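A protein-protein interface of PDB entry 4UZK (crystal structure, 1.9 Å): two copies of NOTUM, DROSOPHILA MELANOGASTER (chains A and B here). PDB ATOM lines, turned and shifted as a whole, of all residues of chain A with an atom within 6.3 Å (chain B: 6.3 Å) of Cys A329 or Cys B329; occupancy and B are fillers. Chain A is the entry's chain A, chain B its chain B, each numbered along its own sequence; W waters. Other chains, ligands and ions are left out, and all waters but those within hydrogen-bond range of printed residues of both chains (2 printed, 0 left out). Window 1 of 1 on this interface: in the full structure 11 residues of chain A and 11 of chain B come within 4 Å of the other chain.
Water W2 lies within hydrogen-bond range of the guanidinium group (NE) of Arg A328 and the side-chain hydroxyl (OG) of Ser B325.
Water W1 bridges the guanidinium group (NE) of Arg B328 (2.7 Å) and the side-chain hydroxyl (OG) of Ser A325 (2.7 Å).
Among the printed residues, pairs that only touch across the chains: Cys A329 with His B332, His A332 with Cys B329, His A332 with Leu B344, Ser A333 with Leu B344, Leu A344 with His B332 and Leu A344 with Ser B333.
Ser A325 touches His B332, and with the chains exchanged His A332 touches Ser B325.
Cys B329 touches its own counterpart, Cys A329.
Cys A329 touches His B332, and with the chains exchanged His A332 touches Cys B329.
His A332 touches Leu B344, and with the chains exchanged Leu A344 touches His B332.
Of the 9 pairs that touch across the chains among the printed residues, 9 have their exchanged pair printed and touching as well.
Of the 13 printed residues of chain A, 5 touch a printed residue of chain B.
Hydrophobic or aromatic side chains of chain A within 4 Å of the printed part of chain B: His A332 and Leu A344.
Printed residues of chain B that touch a printed residue of chain A: Ser B325, Cys B329, His B332, Ser B333 and Leu B344.
Hydrophobic or aromatic side chains of chain B that line the printed part of chain A: His B332 and Leu B344.
Among the printed residues, no Asp or Glu carboxylate lies within 4 Å of a Lys or Arg side-chain nitrogen of the other chain.
Of the printed residues of chain B, Cys A329 touches Cys B329 and His B332.
Of the printed residues of chain A, Cys B329 touches Cys A329 (2.1 Å) and His A332 (3.5 Å).
Of the printed residues of chain A, Ser B333 touches Leu A344.
Printed residues of chain B within 4 Å of Leu A344: His B332 (3.8 Å) and Ser B333 (3.6 Å).
The nearest printed residue of chain B that does not touch Cys A329 is Arg B328 (4.7 Å).
The nearest printed residue of chain B that does not touch Leu A344 is Cys B329 (5.1 Å).
NE2 of His A332 lies within hydrogen-bond range of OG of Ser B325, 2.8 Å away.
The side-chain sulfur (SG) of Cys B329 is disulfide-bonded to the side-chain sulfur (SG) of Cys A329 (2.1 Å).
The side-chain hydroxyl (OG) of Ser A325 sits at hydrogen-bond distance from a ring nitrogen (NE2) of His B332, 2.8 Å away.
The backbone carbonyl oxygen of Trp A330 sits at hydrogen-bond distance from the side-chain hydroxyl of Ser A333, 3.1 Å away.
O of Cys A329 is in hydrogen-bond range of OG of Ser A333.
The backbone carbonyl oxygen (O) of Arg A328 sits close to a ring nitrogen (ND1) of His A332, at 3.4 Å.
The backbone carbonyl oxygen (O) of Arg B328 lies within hydrogen-bond range of a ring nitrogen (ND1) of His B332.
O of Trp B330 is in hydrogen-bond range of OG of Ser B333 (3.3 Å).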
ATOM      1  N   PRO A 324       1.909 -26.788  18.288  1.00  0.00           N
ATOM      2  CA  PRO A 324       2.647 -25.522  18.582  1.00  0.00           C
ATOM      3  C   PRO A 324       3.472 -24.994  17.412  1.00  0.00           C
ATOM      4  O   PRO A 324       3.611 -23.787  17.281  1.00  0.00           O
ATOM      5  CB  PRO A 324       3.572 -25.900  19.739  1.00  0.00           C
ATOM      6  CG  PRO A 324       2.844 -27.060  20.396  1.00  0.00           C
ATOM      7  CD  PRO A 324       2.206 -27.834  19.286  1.00  0.00           C
ATOM      8  N   SER A 325       4.015 -25.905  16.600  1.00  0.00           N
ATOM      9  CA  SER A 325       4.754 -25.514  15.421  1.00  0.00           C
ATOM     10  C   SER A 325       3.861 -24.761  14.422  1.00  0.00           C
ATOM     11  O   SER A 325       4.234 -23.719  13.892  1.00  0.00           O
ATOM     12  CB  SER A 325       5.465 -26.708  14.776  1.00  0.00           C
ATOM     13  OG  SER A 325       6.371 -26.184  13.792  1.00  0.00           O
ATOM     14  N   ALA A 326       2.681 -25.293  14.160  1.00  0.00           N
ATOM     15  CA  ALA A 326       1.679 -24.616  13.313  1.00  0.00           C
ATOM     16  C   ALA A 326       1.273 -23.259  13.846  1.00  0.00           C
ATOM     17  O   ALA A 326       1.145 -22.282  13.070  1.00  0.00           O
ATOM     18  CB  ALA A 326       0.456 -25.486  13.147  1.00  0.00           C
ATOM     19  N   LEU A 327       1.063 -23.161  15.166  1.00  0.00           N
ATOM     20  CA  LEU A 327       0.661 -21.906  15.737  1.00  0.00           C
ATOM     21  C   LEU A 327       1.791 -20.873  15.600  1.00  0.00           C
ATOM     22  O   LEU A 327       1.584 -19.711  15.253  1.00  0.00           O
ATOM     23  CB  LEU A 327       0.291 -22.149  17.195  1.00  0.00           C
ATOM     24  CG  LEU A 327      -0.576 -21.208  17.977  1.00  0.00           C
ATOM     25  CD1 LEU A 327      -1.918 -20.977  17.299  1.00  0.00           C
ATOM     26  CD2 LEU A 327      -0.815 -21.877  19.349  1.00  0.00           C
ATOM     27  N   ARG A 328       3.007 -21.328  15.822  1.00  0.00           N
ATOM     28  CA  ARG A 328       4.191 -20.461  15.670  1.00  0.00           C
ATOM     29  C   ARG A 328       4.323 -19.938  14.216  1.00  0.00           C
ATOM     30  O   ARG A 328       4.629 -18.744  13.997  1.00  0.00           O
ATOM     31  CB  ARG A 328       5.457 -21.232  16.118  1.00  0.00           C
ATOM     32  CG  ARG A 328       6.781 -20.458  16.072  1.00  0.00           C
ATOM     33  CD  ARG A 328       6.716 -19.256  16.995  1.00  0.00           C
ATOM     34  NE  ARG A 328       8.036 -18.806  17.513  1.00  0.00           N
ATOM     35  CZ  ARG A 328       8.203 -17.970  18.531  1.00  0.00           C
ATOM     36  NH1 ARG A 328       7.150 -17.432  19.221  1.00  0.00           N
ATOM     37  NH2 ARG A 328       9.415 -17.729  18.902  1.00  0.00           N
ATOM     38  N   CYS A 329       4.164 -20.809  13.238  1.00  0.00           N
ATOM     39  CA  CYS A 329       4.234 -20.406  11.829  1.00  0.00           C
ATOM     40  C   CYS A 329       3.101 -19.416  11.469  1.00  0.00           C
ATOM     41  O   CYS A 329       3.319 -18.450  10.750  1.00  0.00           O
ATOM     42  CB  CYS A 329       4.252 -21.621  10.898  1.00  0.00           C
ATOM     43  SG  CYS A 329       5.757 -22.603  11.130  1.00  0.00           S
ATOM     44  N   TRP A 330       1.894 -19.605  12.022  1.00  0.00           N
ATOM     45  CA  TRP A 330       0.821 -18.596  11.887  1.00  0.00           C
ATOM     46  C   TRP A 330       1.198 -17.272  12.506  1.00  0.00           C
ATOM     47  O   TRP A 330       1.027 -16.206  11.892  1.00  0.00           O
ATOM     48  CB  TRP A 330      -0.519 -19.132  12.447  1.00  0.00           C
ATOM     49  CG  TRP A 330      -1.573 -18.154  12.734  1.00  0.00           C
ATOM     50  CD1 TRP A 330      -2.442 -17.574  11.846  1.00  0.00           C
ATOM     51  CD2 TRP A 330      -1.937 -17.662  14.022  1.00  0.00           C
ATOM     52  NE1 TRP A 330      -3.334 -16.775  12.520  1.00  0.00           N
ATOM     53  CE2 TRP A 330      -3.045 -16.807  13.847  1.00  0.00           C
ATOM     54  CE3 TRP A 330      -1.463 -17.894  15.299  1.00  0.00           C
ATOM     55  CZ2 TRP A 330      -3.701 -16.207  14.925  1.00  0.00           C
ATOM     56  CZ3 TRP A 330      -2.081 -17.260  16.355  1.00  0.00           C
ATOM     57  CH2 TRP A 330      -3.190 -16.450  16.162  1.00  0.00           C
ATOM     58  N   GLU A 331       1.816 -17.319  13.664  1.00  0.00           N
ATOM     59  CA  GLU A 331       2.245 -16.131  14.318  1.00  0.00           C
ATOM     60  C   GLU A 331       3.197 -15.370  13.408  1.00  0.00           C
ATOM     61  O   GLU A 331       3.011 -14.161  13.187  1.00  0.00           O
ATOM     62  CB  GLU A 331       2.885 -16.522  15.643  1.00  0.00           C
ATOM     63  CG  GLU A 331       3.084 -15.420  16.620  1.00  0.00           C
ATOM     64  CD  GLU A 331       3.862 -15.886  17.852  1.00  0.00           C
ATOM     65  OE1 GLU A 331       4.872 -16.642  17.705  1.00  0.00           O
ATOM     66  OE2 GLU A 331       3.442 -15.492  18.963  1.00  0.00           O
ATOM     67  N   HIS A 332       4.199 -16.064  12.869  1.00  0.00           N
ATOM     68  CA  HIS A 332       5.179 -15.424  11.946  1.00  0.00           C
ATOM     69  C   HIS A 332       4.515 -14.802  10.750  1.00  0.00           C
ATOM     70  O   HIS A 332       4.878 -13.678  10.347  1.00  0.00           O
ATOM     71  CB  HIS A 332       6.189 -16.427  11.410  1.00  0.00           C
ATOM     72  CG  HIS A 332       7.032 -17.070  12.460  1.00  0.00           C
ATOM     73  ND1 HIS A 332       7.172 -16.558  13.715  1.00  0.00           N
ATOM     74  CD2 HIS A 332       7.826 -18.160  12.409  1.00  0.00           C
ATOM     75  CE1 HIS A 332       7.995 -17.309  14.418  1.00  0.00           C
ATOM     76  NE2 HIS A 332       8.400 -18.293  13.648  1.00  0.00           N
ATOM     77  N   SER A 333       3.556 -15.521  10.161  1.00  0.00           N
ATOM     78  CA  SER A 333       2.976 -15.085   8.916  1.00  0.00           C
ATOM     79  C   SER A 333       1.977 -13.932   9.092  1.00  0.00           C
ATOM     80  O   SER A 333       1.692 -13.230   8.143  1.00  0.00           O
ATOM     81  CB  SER A 333       2.369 -16.276   8.157  1.00  0.00           C
ATOM     82  OG  SER A 333       1.169 -16.562   8.769  1.00  0.00           O
ATOM     83  N   THR A 334       1.511 -13.664  10.308  1.00  0.00           N
ATOM     84  CA  THR A 334       0.559 -12.605  10.569  1.00  0.00           C
ATOM     85  C   THR A 334       1.195 -11.475  11.377  1.00  0.00           C
ATOM     86  O   THR A 334       0.503 -10.745  12.049  1.00  0.00           O
ATOM     87  CB  THR A 334      -0.690 -13.132  11.305  1.00  0.00           C
ATOM     88  OG1 THR A 334      -0.324 -13.826  12.504  1.00  0.00           O
ATOM     89  CG2 THR A 334      -1.422 -14.094  10.400  1.00  0.00           C
ATOM     90  N   GLY A 343      -2.207 -18.518   5.973  1.00  0.00           N
ATOM     91  CA  GLY A 343      -1.565 -19.395   6.955  1.00  0.00           C
ATOM     92  C   GLY A 343      -1.667 -20.856   6.549  1.00  0.00           C
ATOM     93  O   GLY A 343      -1.963 -21.172   5.399  1.00  0.00           O
ATOM     94  N   LEU A 344      -1.420 -21.765   7.481  1.00  0.00           N
ATOM     95  CA  LEU A 344      -1.449 -23.175   7.145  1.00  0.00           C
ATOM     96  C   LEU A 344      -2.860 -23.710   7.338  1.00  0.00           C
ATOM     97  O   LEU A 344      -3.470 -23.493   8.382  1.00  0.00           O
ATOM     98  CB  LEU A 344      -0.500 -24.003   8.034  1.00  0.00           C
ATOM     99  CG  LEU A 344       1.012 -23.784   7.954  1.00  0.00           C
ATOM    100  CD1 LEU A 344       1.719 -24.476   9.104  1.00  0.00           C
ATOM    101  CD2 LEU A 344       1.593 -24.273   6.639  1.00  0.00           C
ATOM    102  N   TRP B  92      16.251 -30.424  12.306  1.00  0.00           N
ATOM    103  CA  TRP B  92      16.787 -31.418  11.393  1.00  0.00           C
ATOM    104  C   TRP B  92      17.895 -32.261  12.022  1.00  0.00           C
ATOM    105  O   TRP B  92      18.545 -32.997  11.335  1.00  0.00           O
ATOM    106  CB  TRP B  92      17.223 -30.739  10.092  1.00  0.00           C
ATOM    107  CG  TRP B  92      16.082 -30.042   9.466  1.00  0.00           C
ATOM    108  CD1 TRP B  92      15.092 -30.610   8.712  1.00  0.00           C
ATOM    109  CD2 TRP B  92      15.715 -28.664   9.621  1.00  0.00           C
ATOM    110  NE1 TRP B  92      14.129 -29.650   8.373  1.00  0.00           N
ATOM    111  CE2 TRP B  92      14.492 -28.459   8.917  1.00  0.00           C
ATOM    112  CE3 TRP B  92      16.302 -27.572  10.260  1.00  0.00           C
ATOM    113  CZ2 TRP B  92      13.874 -27.193   8.818  1.00  0.00           C
ATOM    114  CZ3 TRP B  92      15.666 -26.306  10.167  1.00  0.00           C
ATOM    115  CH2 TRP B  92      14.478 -26.145   9.441  1.00  0.00           C
ATOM    116  N   PRO B 324      16.361 -20.937  11.507  1.00  0.00           N
ATOM    117  CA  PRO B 324      15.731 -22.250  11.505  1.00  0.00           C
ATOM    118  C   PRO B 324      14.214 -22.213  11.605  1.00  0.00           C
ATOM    119  O   PRO B 324      13.576 -23.080  11.016  1.00  0.00           O
ATOM    120  CB  PRO B 324      16.347 -22.947  12.751  1.00  0.00           C
ATOM    121  CG  PRO B 324      17.617 -22.227  12.953  1.00  0.00           C
ATOM    122  CD  PRO B 324      17.341 -20.806  12.606  1.00  0.00           C
ATOM    123  N   SER B 325      13.643 -21.267  12.374  1.00  0.00           N
ATOM    124  CA  SER B 325      12.209 -21.208  12.533  1.00  0.00           C
ATOM    125  C   SER B 325      11.553 -20.804  11.200  1.00  0.00           C
ATOM    126  O   SER B 325      10.529 -21.386  10.802  1.00  0.00           O
ATOM    127  CB  SER B 325      11.804 -20.278  13.674  1.00  0.00           C
ATOM    128  OG  SER B 325      10.403 -20.293  13.833  1.00  0.00           O
ATOM    129  N   ALA B 326      12.181 -19.888  10.480  1.00  0.00           N
ATOM    130  CA  ALA B 326      11.674 -19.486   9.137  1.00  0.00           C
ATOM    131  C   ALA B 326      11.779 -20.620   8.138  1.00  0.00           C
ATOM    132  O   ALA B 326      10.841 -20.868   7.405  1.00  0.00           O
ATOM    133  CB  ALA B 326      12.439 -18.272   8.641  1.00  0.00           C
ATOM    134  N   LEU B 327      12.898 -21.357   8.152  1.00  0.00           N
ATOM    135  CA  LEU B 327      13.065 -22.505   7.269  1.00  0.00           C
ATOM    136  C   LEU B 327      12.036 -23.584   7.580  1.00  0.00           C
ATOM    137  O   LEU B 327      11.481 -24.192   6.676  1.00  0.00           O
ATOM    138  CB  LEU B 327      14.479 -23.066   7.404  1.00  0.00           C
ATOM    139  CG  LEU B 327      14.949 -24.057   6.365  1.00  0.00           C
ATOM    140  CD1 LEU B 327      14.974 -23.408   4.993  1.00  0.00           C
ATOM    141  CD2 LEU B 327      16.318 -24.565   6.756  1.00  0.00           C
ATOM    142  N   ARG B 328      11.805 -23.818   8.858  1.00  0.00           N
ATOM    143  CA  ARG B 328      10.768 -24.814   9.268  1.00  0.00           C
ATOM    144  C   ARG B 328       9.369 -24.401   8.801  1.00  0.00           C
ATOM    145  O   ARG B 328       8.609 -25.235   8.312  1.00  0.00           O
ATOM    146  CB  ARG B 328      10.874 -24.999  10.799  1.00  0.00           C
ATOM    147  CG  ARG B 328       9.906 -26.000  11.395  1.00  0.00           C
ATOM    148  CD  ARG B 328      10.259 -27.375  10.865  1.00  0.00           C
ATOM    149  NE  ARG B 328       9.895 -28.429  11.827  1.00  0.00           N
ATOM    150  CZ  ARG B 328      10.214 -29.704  11.675  1.00  0.00           C
ATOM    151  NH1 ARG B 328      10.876 -30.139  10.573  1.00  0.00           N
ATOM    152  NH2 ARG B 328       9.914 -30.518  12.642  1.00  0.00           N
ATOM    153  N   CYS B 329       8.999 -23.136   8.964  1.00  0.00           N
ATOM    154  CA  CYS B 329       7.705 -22.678   8.484  1.00  0.00           C
ATOM    155  C   CYS B 329       7.565 -22.792   6.966  1.00  0.00           C
ATOM    156  O   CYS B 329       6.527 -23.205   6.452  1.00  0.00           O
ATOM    157  CB  CYS B 329       7.453 -21.283   8.953  1.00  0.00           C
ATOM    158  SG  CYS B 329       7.284 -21.242  10.746  1.00  0.00           S
ATOM    159  N   TRP B 330       8.640 -22.480   6.237  1.00  0.00           N
ATOM    160  CA  TRP B 330       8.608 -22.698   4.792  1.00  0.00           C
ATOM    161  C   TRP B 330       8.440 -24.159   4.434  1.00  0.00           C
ATOM    162  O   TRP B 330       7.698 -24.540   3.507  1.00  0.00           O
ATOM    163  CB  TRP B 330       9.903 -22.165   4.218  1.00  0.00           C
ATOM    164  CG  TRP B 330      10.265 -22.657   2.807  1.00  0.00           C
ATOM    165  CD1 TRP B 330       9.730 -22.216   1.632  1.00  0.00           C
ATOM    166  CD2 TRP B 330      11.271 -23.575   2.467  1.00  0.00           C
ATOM    167  NE1 TRP B 330      10.369 -22.810   0.568  1.00  0.00           N
ATOM    168  CE2 TRP B 330      11.306 -23.665   1.054  1.00  0.00           C
ATOM    169  CE3 TRP B 330      12.119 -24.387   3.207  1.00  0.00           C
ATOM    170  CZ2 TRP B 330      12.188 -24.485   0.380  1.00  0.00           C
ATOM    171  CZ3 TRP B 330      13.024 -25.202   2.510  1.00  0.00           C
ATOM    172  CH2 TRP B 330      13.048 -25.217   1.107  1.00  0.00           C
ATOM    173  N   GLU B 331       9.131 -25.020   5.153  1.00  0.00           N
ATOM    174  CA  GLU B 331       8.966 -26.428   4.955  1.00  0.00           C
ATOM    175  C   GLU B 331       7.480 -26.851   5.144  1.00  0.00           C
ATOM    176  O   GLU B 331       6.881 -27.542   4.280  1.00  0.00           O
ATOM    177  CB  GLU B 331       9.890 -27.169   5.918  1.00  0.00           C
ATOM    178  CG  GLU B 331      10.147 -28.601   5.624  1.00  0.00           C
ATOM    179  CD  GLU B 331      10.882 -29.309   6.781  1.00  0.00           C
ATOM    180  OE1 GLU B 331      10.441 -29.148   7.947  1.00  0.00           O
ATOM    181  OE2 GLU B 331      11.860 -30.044   6.525  1.00  0.00           O
ATOM    182  N   HIS B 332       6.864 -26.424   6.238  1.00  0.00           N
ATOM    183  CA  HIS B 332       5.446 -26.771   6.455  1.00  0.00           C
ATOM    184  C   HIS B 332       4.567 -26.247   5.304  1.00  0.00           C
ATOM    185  O   HIS B 332       3.653 -26.930   4.813  1.00  0.00           O
ATOM    186  CB  HIS B 332       4.907 -26.087   7.708  1.00  0.00           C
ATOM    187  CG  HIS B 332       5.538 -26.523   8.982  1.00  0.00           C
ATOM    188  ND1 HIS B 332       6.366 -27.604   9.088  1.00  0.00           N
ATOM    189  CD2 HIS B 332       5.444 -26.002  10.226  1.00  0.00           C
ATOM    190  CE1 HIS B 332       6.775 -27.732  10.333  1.00  0.00           C
ATOM    191  NE2 HIS B 332       6.203 -26.788  11.044  1.00  0.00           N
ATOM    192  N   SER B 333       4.841 -25.029   4.874  1.00  0.00           N
ATOM    193  CA  SER B 333       3.983 -24.381   3.890  1.00  0.00           C
ATOM    194  C   SER B 333       4.143 -24.929   2.459  1.00  0.00           C
ATOM    195  O   SER B 333       3.242 -24.737   1.634  1.00  0.00           O
ATOM    196  CB  SER B 333       4.082 -22.844   3.982  1.00  0.00           C
ATOM    197  OG  SER B 333       5.163 -22.386   3.269  1.00  0.00           O
ATOM    198  N   THR B 334       5.234 -25.646   2.186  1.00  0.00           N
ATOM    199  CA  THR B 334       5.535 -26.183   0.863  1.00  0.00           C
ATOM    200  C   THR B 334       5.393 -27.698   0.850  1.00  0.00           C
ATOM    201  O   THR B 334       5.916 -28.373  -0.046  1.00  0.00           O
ATOM    202  CB  THR B 334       6.960 -25.800   0.379  1.00  0.00           C
ATOM    203  OG1 THR B 334       7.929 -26.202   1.363  1.00  0.00           O
ATOM    204  CG2 THR B 334       7.029 -24.331   0.144  1.00  0.00           C
ATOM    205  N   LEU B 344       7.067 -16.866   3.552  1.00  0.00           N
ATOM    206  CA  LEU B 344       7.547 -15.801   4.455  1.00  0.00           C
ATOM    207  C   LEU B 344       8.684 -15.029   3.798  1.00  0.00           C
ATOM    208  O   LEU B 344       9.706 -15.625   3.450  1.00  0.00           O
ATOM    209  CB  LEU B 344       8.098 -16.326   5.801  1.00  0.00           C
ATOM    210  CG  LEU B 344       7.195 -16.895   6.904  1.00  0.00           C
ATOM    211  CD1 LEU B 344       8.045 -17.354   8.088  1.00  0.00           C
ATOM    212  CD2 LEU B 344       6.103 -15.921   7.370  1.00  0.00           C
HETATM  213  O   HOH W   1       8.228 -28.134  13.905  1.00  0.00           O
HETATM  214  O   HOH W   2      10.341 -19.702  16.503  1.00  0.00           O
